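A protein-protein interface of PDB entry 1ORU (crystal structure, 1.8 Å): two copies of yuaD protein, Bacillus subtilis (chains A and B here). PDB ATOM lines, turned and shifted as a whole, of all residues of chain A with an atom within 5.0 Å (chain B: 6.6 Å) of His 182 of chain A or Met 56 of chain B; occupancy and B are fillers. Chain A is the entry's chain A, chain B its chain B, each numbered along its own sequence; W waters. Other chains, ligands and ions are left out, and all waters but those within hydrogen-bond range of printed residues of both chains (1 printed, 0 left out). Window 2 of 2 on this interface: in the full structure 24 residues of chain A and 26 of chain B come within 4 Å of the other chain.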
ATOM      1  N   TRP A   5      17.993 -13.184   2.691  1.00  0.00           N
ATOM      2  CA  TRP A   5      18.986 -12.372   2.001  1.00  0.00           C
ATOM      3  C   TRP A   5      18.443 -10.971   1.745  1.00  0.00           C
ATOM      4  O   TRP A   5      17.633 -10.788   0.842  1.00  0.00           O
ATOM      5  CB  TRP A   5      19.345 -13.009   0.648  1.00  0.00           C
ATOM      6  CG  TRP A   5      20.096 -14.295   0.745  1.00  0.00           C
ATOM      7  CD1 TRP A   5      19.673 -15.536   0.341  1.00  0.00           C
ATOM      8  CD2 TRP A   5      21.388 -14.481   1.321  1.00  0.00           C
ATOM      9  NE1 TRP A   5      20.627 -16.483   0.639  1.00  0.00           N
ATOM     10  CE2 TRP A   5      21.691 -15.859   1.239  1.00  0.00           C
ATOM     11  CE3 TRP A   5      22.322 -13.616   1.900  1.00  0.00           C
ATOM     12  CZ2 TRP A   5      22.888 -16.391   1.720  1.00  0.00           C
ATOM     13  CZ3 TRP A   5      23.509 -14.145   2.377  1.00  0.00           C
ATOM     14  CH2 TRP A   5      23.782 -15.518   2.283  1.00  0.00           C
ATOM     15  N   LYS A   6      18.866  -9.986   2.532  1.00  0.00           N
ATOM     16  CA  LYS A   6      18.402  -8.620   2.290  1.00  0.00           C
ATOM     17  C   LYS A   6      19.515  -7.898   1.537  1.00  0.00           C
ATOM     18  O   LYS A   6      20.664  -7.879   1.979  1.00  0.00           O
ATOM     19  CB  LYS A   6      18.089  -7.887   3.601  1.00  0.00           C
ATOM     20  CG  LYS A   6      19.285  -7.648   4.511  1.00  0.00           C
ATOM     21  CD  LYS A   6      18.924  -6.760   5.707  1.00  0.00           C
ATOM     22  CE  LYS A   6      20.078  -6.675   6.709  1.00  0.00           C
ATOM     23  NZ  LYS A   6      19.798  -5.783   7.872  1.00  0.00           N
ATOM     24  N   ARG A   7      19.175  -7.317   0.392  1.00  0.00           N
ATOM     25  CA  ARG A   7      20.164  -6.616  -0.417  1.00  0.00           C
ATOM     26  C   ARG A   7      20.219  -5.115  -0.193  1.00  0.00           C
ATOM     27  O   ARG A   7      19.195  -4.465   0.004  1.00  0.00           O
ATOM     28  CB  ARG A   7      19.912  -6.884  -1.903  1.00  0.00           C
ATOM     29  CG  ARG A   7      20.241  -8.296  -2.338  1.00  0.00           C
ATOM     30  CD  ARG A   7      19.693  -8.580  -3.721  1.00  0.00           C
ATOM     31  NE  ARG A   7      18.244  -8.421  -3.746  1.00  0.00           N
ATOM     32  CZ  ARG A   7      17.481  -8.676  -4.802  1.00  0.00           C
ATOM     33  NH1 ARG A   7      18.028  -9.106  -5.932  1.00  0.00           N
ATOM     34  NH2 ARG A   7      16.168  -8.499  -4.725  1.00  0.00           N
ATOM     35  N   GLY A 112      28.374 -15.383   6.246  1.00  0.00           N
ATOM     36  CA  GLY A 112      27.510 -15.938   5.217  1.00  0.00           C
ATOM     37  C   GLY A 112      27.019 -14.859   4.267  1.00  0.00           C
ATOM     38  O   GLY A 112      26.518 -15.155   3.180  1.00  0.00           O
ATOM     39  N   SER A 113      27.138 -13.601   4.685  1.00  0.00           N
ATOM     40  CA  SER A 113      26.735 -12.481   3.844  1.00  0.00           C
ATOM     41  C   SER A 113      27.763 -12.372   2.722  1.00  0.00           C
ATOM     42  O   SER A 113      28.893 -12.833   2.863  1.00  0.00           O
ATOM     43  CB  SER A 113      26.725 -11.170   4.642  1.00  0.00           C
ATOM     44  OG  SER A 113      25.763 -11.195   5.686  1.00  0.00           O
ATOM     45  N   ARG A 114      27.366 -11.760   1.614  1.00  0.00           N
ATOM     46  CA  ARG A 114      28.253 -11.571   0.472  1.00  0.00           C
ATOM     47  C   ARG A 114      28.334 -10.105   0.087  1.00  0.00           C
ATOM     48  O   ARG A 114      27.356  -9.369   0.228  1.00  0.00           O
ATOM     49  CB  ARG A 114      27.733 -12.342  -0.745  1.00  0.00           C
ATOM     50  CG  ARG A 114      28.263 -13.741  -0.900  1.00  0.00           C
ATOM     51  CD  ARG A 114      27.681 -14.701   0.112  1.00  0.00           C
ATOM     52  NE  ARG A 114      27.986 -16.066  -0.299  1.00  0.00           N
ATOM     53  CZ  ARG A 114      27.326 -17.140   0.111  1.00  0.00           C
ATOM     54  NH1 ARG A 114      26.312 -17.020   0.965  1.00  0.00           N
ATOM     55  NH2 ARG A 114      27.665 -18.337  -0.357  1.00  0.00           N
ATOM     56  N   ILE A 115      29.508  -9.689  -0.381  1.00  0.00           N
ATOM     57  CA  ILE A 115      29.743  -8.328  -0.865  1.00  0.00           C
ATOM     58  C   ILE A 115      30.248  -8.519  -2.294  1.00  0.00           C
ATOM     59  O   ILE A 115      31.327  -9.083  -2.514  1.00  0.00           O
ATOM     60  CB  ILE A 115      30.821  -7.589  -0.046  1.00  0.00           C
ATOM     61  CG1 ILE A 115      30.348  -7.426   1.401  1.00  0.00           C
ATOM     62  CG2 ILE A 115      31.098  -6.220  -0.674  1.00  0.00           C
ATOM     63  CD1 ILE A 115      31.377  -6.791   2.319  1.00  0.00           C
ATOM     64  N   ILE A 116      29.470  -8.044  -3.261  1.00  0.00           N
ATOM     65  CA  ILE A 116      29.808  -8.218  -4.666  1.00  0.00           C
ATOM     66  C   ILE A 116      30.115  -6.912  -5.392  1.00  0.00           C
ATOM     67  O   ILE A 116      29.402  -5.917  -5.242  1.00  0.00           O
ATOM     68  CB  ILE A 116      28.663  -8.965  -5.380  1.00  0.00           C
ATOM     69  CG1 ILE A 116      28.379 -10.276  -4.641  1.00  0.00           C
ATOM     70  CG2 ILE A 116      29.030  -9.239  -6.837  1.00  0.00           C
ATOM     71  CD1 ILE A 116      27.322 -11.145  -5.302  1.00  0.00           C
ATOM     72  N   GLU A 180      27.342  -4.367  -3.913  1.00  0.00           N
ATOM     73  CA  GLU A 180      26.049  -4.954  -3.600  1.00  0.00           C
ATOM     74  C   GLU A 180      26.248  -5.856  -2.392  1.00  0.00           C
ATOM     75  O   GLU A 180      26.994  -6.830  -2.465  1.00  0.00           O
ATOM     76  CB  GLU A 180      25.565  -5.789  -4.785  1.00  0.00           C
ATOM     77  CG  GLU A 180      24.134  -6.264  -4.683  1.00  0.00           C
ATOM     78  CD  GLU A 180      23.141  -5.165  -4.994  1.00  0.00           C
ATOM     79  OE1 GLU A 180      21.924  -5.452  -5.013  1.00  0.00           O
ATOM     80  OE2 GLU A 180      23.581  -4.016  -5.224  1.00  0.00           O
ATOM     81  N   VAL A 181      25.595  -5.530  -1.280  1.00  0.00           N
ATOM     82  CA  VAL A 181      25.732  -6.339  -0.076  1.00  0.00           C
ATOM     83  C   VAL A 181      24.515  -7.237   0.093  1.00  0.00           C
ATOM     84  O   VAL A 181      23.378  -6.764   0.059  1.00  0.00           O
ATOM     85  CB  VAL A 181      25.889  -5.451   1.183  1.00  0.00           C
ATOM     86  CG1 VAL A 181      26.028  -6.323   2.434  1.00  0.00           C
ATOM     87  CG2 VAL A 181      27.112  -4.544   1.025  1.00  0.00           C
ATOM     88  N   HIS A 182      24.765  -8.538   0.229  1.00  0.00           N
ATOM     89  CA  HIS A 182      23.707  -9.520   0.437  1.00  0.00           C
ATOM     90  C   HIS A 182      23.850  -9.926   1.898  1.00  0.00           C
ATOM     91  O   HIS A 182      24.693 -10.762   2.249  1.00  0.00           O
ATOM     92  CB  HIS A 182      23.909 -10.716  -0.495  1.00  0.00           C
ATOM     93  CG  HIS A 182      23.852 -10.356  -1.947  1.00  0.00           C
ATOM     94  ND1 HIS A 182      22.699 -10.454  -2.695  1.00  0.00           N
ATOM     95  CD2 HIS A 182      24.794  -9.845  -2.773  1.00  0.00           C
ATOM     96  CE1 HIS A 182      22.932 -10.018  -3.921  1.00  0.00           C
ATOM     97  NE2 HIS A 182      24.197  -9.640  -3.994  1.00  0.00           N
ATOM     98  N   SER A 183      23.044  -9.296   2.748  1.00  0.00           N
ATOM     99  CA  SER A 183      23.089  -9.533   4.186  1.00  0.00           C
ATOM    100  C   SER A 183      22.324 -10.783   4.606  1.00  0.00           C
ATOM    101  O   SER A 183      21.112 -10.882   4.409  1.00  0.00           O
ATOM    102  CB  SER A 183      22.547  -8.302   4.919  1.00  0.00           C
ATOM    103  OG  SER A 183      22.842  -8.350   6.302  1.00  0.00           O
ATOM    104  N   TYR A 184      23.046 -11.735   5.193  1.00  0.00           N
ATOM    105  CA  TYR A 184      22.460 -12.995   5.639  1.00  0.00           C
ATOM    106  C   TYR A 184      21.530 -12.807   6.836  1.00  0.00           C
ATOM    107  O   TYR A 184      21.839 -12.049   7.759  1.00  0.00           O
ATOM    108  CB  TYR A 184      23.569 -13.984   6.005  1.00  0.00           C
ATOM    109  CG  TYR A 184      23.068 -15.330   6.488  1.00  0.00           C
ATOM    110  CD1 TYR A 184      22.353 -16.178   5.639  1.00  0.00           C
ATOM    111  CD2 TYR A 184      23.318 -15.762   7.791  1.00  0.00           C
ATOM    112  CE1 TYR A 184      21.900 -17.424   6.078  1.00  0.00           C
ATOM    113  CE2 TYR A 184      22.869 -17.008   8.240  1.00  0.00           C
ATOM    114  CZ  TYR A 184      22.163 -17.832   7.377  1.00  0.00           C
ATOM    115  OH  TYR A 184      21.724 -19.065   7.811  1.00  0.00           O
ATOM    116  N   GLY B  51      24.617 -22.682  -6.860  1.00  0.00           N
ATOM    117  CA  GLY B  51      23.306 -23.266  -7.044  1.00  0.00           C
ATOM    118  C   GLY B  51      22.267 -22.495  -6.257  1.00  0.00           C
ATOM    119  O   GLY B  51      22.475 -21.336  -5.904  1.00  0.00           O
ATOM    120  N   ARG B  53      21.572 -22.589  -3.301  1.00  0.00           N
ATOM    121  CA  ARG B  53      22.057 -22.184  -1.980  1.00  0.00           C
ATOM    122  C   ARG B  53      22.828 -20.867  -2.013  1.00  0.00           C
ATOM    123  O   ARG B  53      22.961 -20.190  -0.992  1.00  0.00           O
ATOM    124  CB  ARG B  53      22.954 -23.267  -1.378  1.00  0.00           C
ATOM    125  CG  ARG B  53      22.252 -24.576  -1.062  1.00  0.00           C
ATOM    126  CD  ARG B  53      23.268 -25.608  -0.609  1.00  0.00           C
ATOM    127  NE  ARG B  53      22.673 -26.919  -0.378  1.00  0.00           N
ATOM    128  CZ  ARG B  53      21.850 -27.198   0.626  1.00  0.00           C
ATOM    129  NH1 ARG B  53      21.522 -26.253   1.494  1.00  0.00           N
ATOM    130  NH2 ARG B  53      21.371 -28.426   0.773  1.00  0.00           N
ATOM    131  N   GLU B  54      23.340 -20.514  -3.185  1.00  0.00           N
ATOM    132  CA  GLU B  54      24.090 -19.270  -3.354  1.00  0.00           C
ATOM    133  C   GLU B  54      23.403 -18.466  -4.458  1.00  0.00           C
ATOM    134  O   GLU B  54      23.987 -18.206  -5.514  1.00  0.00           O
ATOM    135  CB  GLU B  54      25.540 -19.577  -3.746  1.00  0.00           C
ATOM    136  CG  GLU B  54      26.262 -20.560  -2.814  1.00  0.00           C
ATOM    137  CD  GLU B  54      26.125 -22.015  -3.253  1.00  0.00           C
ATOM    138  OE1 GLU B  54      25.399 -22.277  -4.240  1.00  0.00           O
ATOM    139  OE2 GLU B  54      26.749 -22.897  -2.617  1.00  0.00           O
ATOM    140  N   PRO B  55      22.154 -18.031  -4.209  1.00  0.00           N
ATOM    141  CA  PRO B  55      21.355 -17.264  -5.170  1.00  0.00           C
ATOM    142  C   PRO B  55      21.900 -15.937  -5.681  1.00  0.00           C
ATOM    143  O   PRO B  55      21.387 -15.408  -6.670  1.00  0.00           O
ATOM    144  CB  PRO B  55      20.013 -17.111  -4.455  1.00  0.00           C
ATOM    145  CG  PRO B  55      20.413 -17.026  -3.020  1.00  0.00           C
ATOM    146  CD  PRO B  55      21.461 -18.117  -2.908  1.00  0.00           C
ATOM    147  N   MET B  56      22.926 -15.391  -5.030  1.00  0.00           N
ATOM    148  CA  MET B  56      23.480 -14.128  -5.499  1.00  0.00           C
ATOM    149  C   MET B  56      24.388 -14.346  -6.713  1.00  0.00           C
ATOM    150  O   MET B  56      24.891 -13.391  -7.302  1.00  0.00           O
ATOM    151  CB  MET B  56      24.230 -13.389  -4.374  1.00  0.00           C
ATOM    152  CG  MET B  56      25.457 -14.087  -3.793  1.00  0.00           C
ATOM    153  SD  MET B  56      25.073 -15.615  -2.670  1.00  0.00           S
ATOM    154  CE  MET B  56      23.978 -14.763  -1.316  1.00  0.00           C
ATOM    155  N   PHE B  57      24.573 -15.604  -7.098  1.00  0.00           N
ATOM    156  CA  PHE B  57      25.394 -15.942  -8.261  1.00  0.00           C
ATOM    157  C   PHE B  57      24.502 -16.658  -9.269  1.00  0.00           C
ATOM    158  O   PHE B  57      23.514 -17.291  -8.884  1.00  0.00           O
ATOM    159  CB  PHE B  57      26.527 -16.890  -7.863  1.00  0.00           C
ATOM    160  CG  PHE B  57      27.456 -16.333  -6.830  1.00  0.00           C
ATOM    161  CD1 PHE B  57      28.380 -15.344  -7.165  1.00  0.00           C
ATOM    162  CD2 PHE B  57      27.420 -16.807  -5.520  1.00  0.00           C
ATOM    163  CE1 PHE B  57      29.261 -14.833  -6.215  1.00  0.00           C
ATOM    164  CE2 PHE B  57      28.298 -16.307  -4.554  1.00  0.00           C
ATOM    165  CZ  PHE B  57      29.222 -15.317  -4.904  1.00  0.00           C
ATOM    166  N   SER B  58      24.832 -16.566 -10.553  1.00  0.00           N
ATOM    167  CA  SER B  58      24.039 -17.272 -11.552  1.00  0.00           C
ATOM    168  C   SER B  58      24.416 -18.750 -11.413  1.00  0.00           C
ATOM    169  O   SER B  58      25.570 -19.082 -11.114  1.00  0.00           O
ATOM    170  CB  SER B  58      24.347 -16.766 -12.965  1.00  0.00           C
ATOM    171  OG  SER B  58      25.673 -17.076 -13.348  1.00  0.00           O
HETATM  172  O   HOH W   1      24.903 -19.543   1.033  1.00  0.00           O
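Pro 55 of chain B touches Trp 5 of chain A. CE of Met 56 of chain B touches CE2 of Trp 5 of chain A, at 3.6 Å. Arg 114 of chain A touches Glu 54 of chain B. Ile 116 of chain A touches Met 56 of chain B (CD1 to CG, 3.8 Å). CB of Met 56 of chain B touches CE1 of His 182 of chain A (3.6 Å).
No position is printed for both chains.
The backbone carbonyl oxygen of Gly 112 of chain A sits at hydrogen-bond distance from the guanidinium group of Arg 114 of chain A, at 2.9 Å. The backbone NH (N) of His 182 of chain A is in hydrogen-bond range of the backbone carbonyl oxygen (O) of Arg 114 of chain A (2.7 Å). The backbone NH (N) of Ile 116 of chain A sits at hydrogen-bond distance from the backbone carbonyl oxygen (O) of Glu 180 of chain A (2.9 Å). The side-chain carboxylate (OE1) of Glu 54 of chain B sits at hydrogen-bond distance from the backbone NH (N) of Gly 51 of chain B (2.8 Å).
Printed residues of chain B within 4 Å of Trp 5 of chain A: Pro 55 (3.7 Å) and Met 56 (3.6 Å). Printed residues of chain B within 4 Å of Arg 114 of chain A: Glu 54 and Met 56. Of the printed residues of chain B, Ile 116 of chain A touches Met 56 (3.8 Å). His 182 of chain A touches just one residue of chain B: Met 56 (3.6 Å). Printed residues of chain A within 4 Å of Glu 54 of chain B: Arg 114 (3.6 Å). Printed residues of chain A within 4 Å of Pro 55 of chain B: Trp 5. Met 56 of chain B touches just these residues of chain A: Trp 5, Arg 114, Ile 116 and His 182. The nearest residue of chain B that does not touch His 182 of chain A is Pro 55 of chain B (6.2 Å). The nearest printed residue of chain A that does not touch Met 56 of chain B is Gly 112 of chain A (5.2 Å).
Water W1 lies within hydrogen-bond range of O of Arg 53 of chain B (2.9 Å) and NH1 of Arg 114 of chain A (2.9 Å).
Of the 7 printed residues of chain B, 3 touch a printed residue of chain A. Printed residues of chain B that touch a printed residue of chain A: Glu 54, Pro 55 and Met 56. Hydrophobic or aromatic side chains of chain B within 4 Å of the printed part of chain A: Pro 55 and Met 56. Along chain B the printed residues that touch a printed residue of chain A span positions 54 to 56. Hydrophobic or aromatic side chains of chain A that line the printed part of chain B: Trp 5, Ile 116 and His 182. Among the printed residues, no Asp or Glu carboxylate lies within 4 Å of a Lys or Arg side-chain nitrogen of the other chain.
The side-chain sulfur (SD) of Met 56 of chain B sits at hydrogen-bond distance from the guanidinium group (NE) of Arg 114 of chain A, 3.8 Å away.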
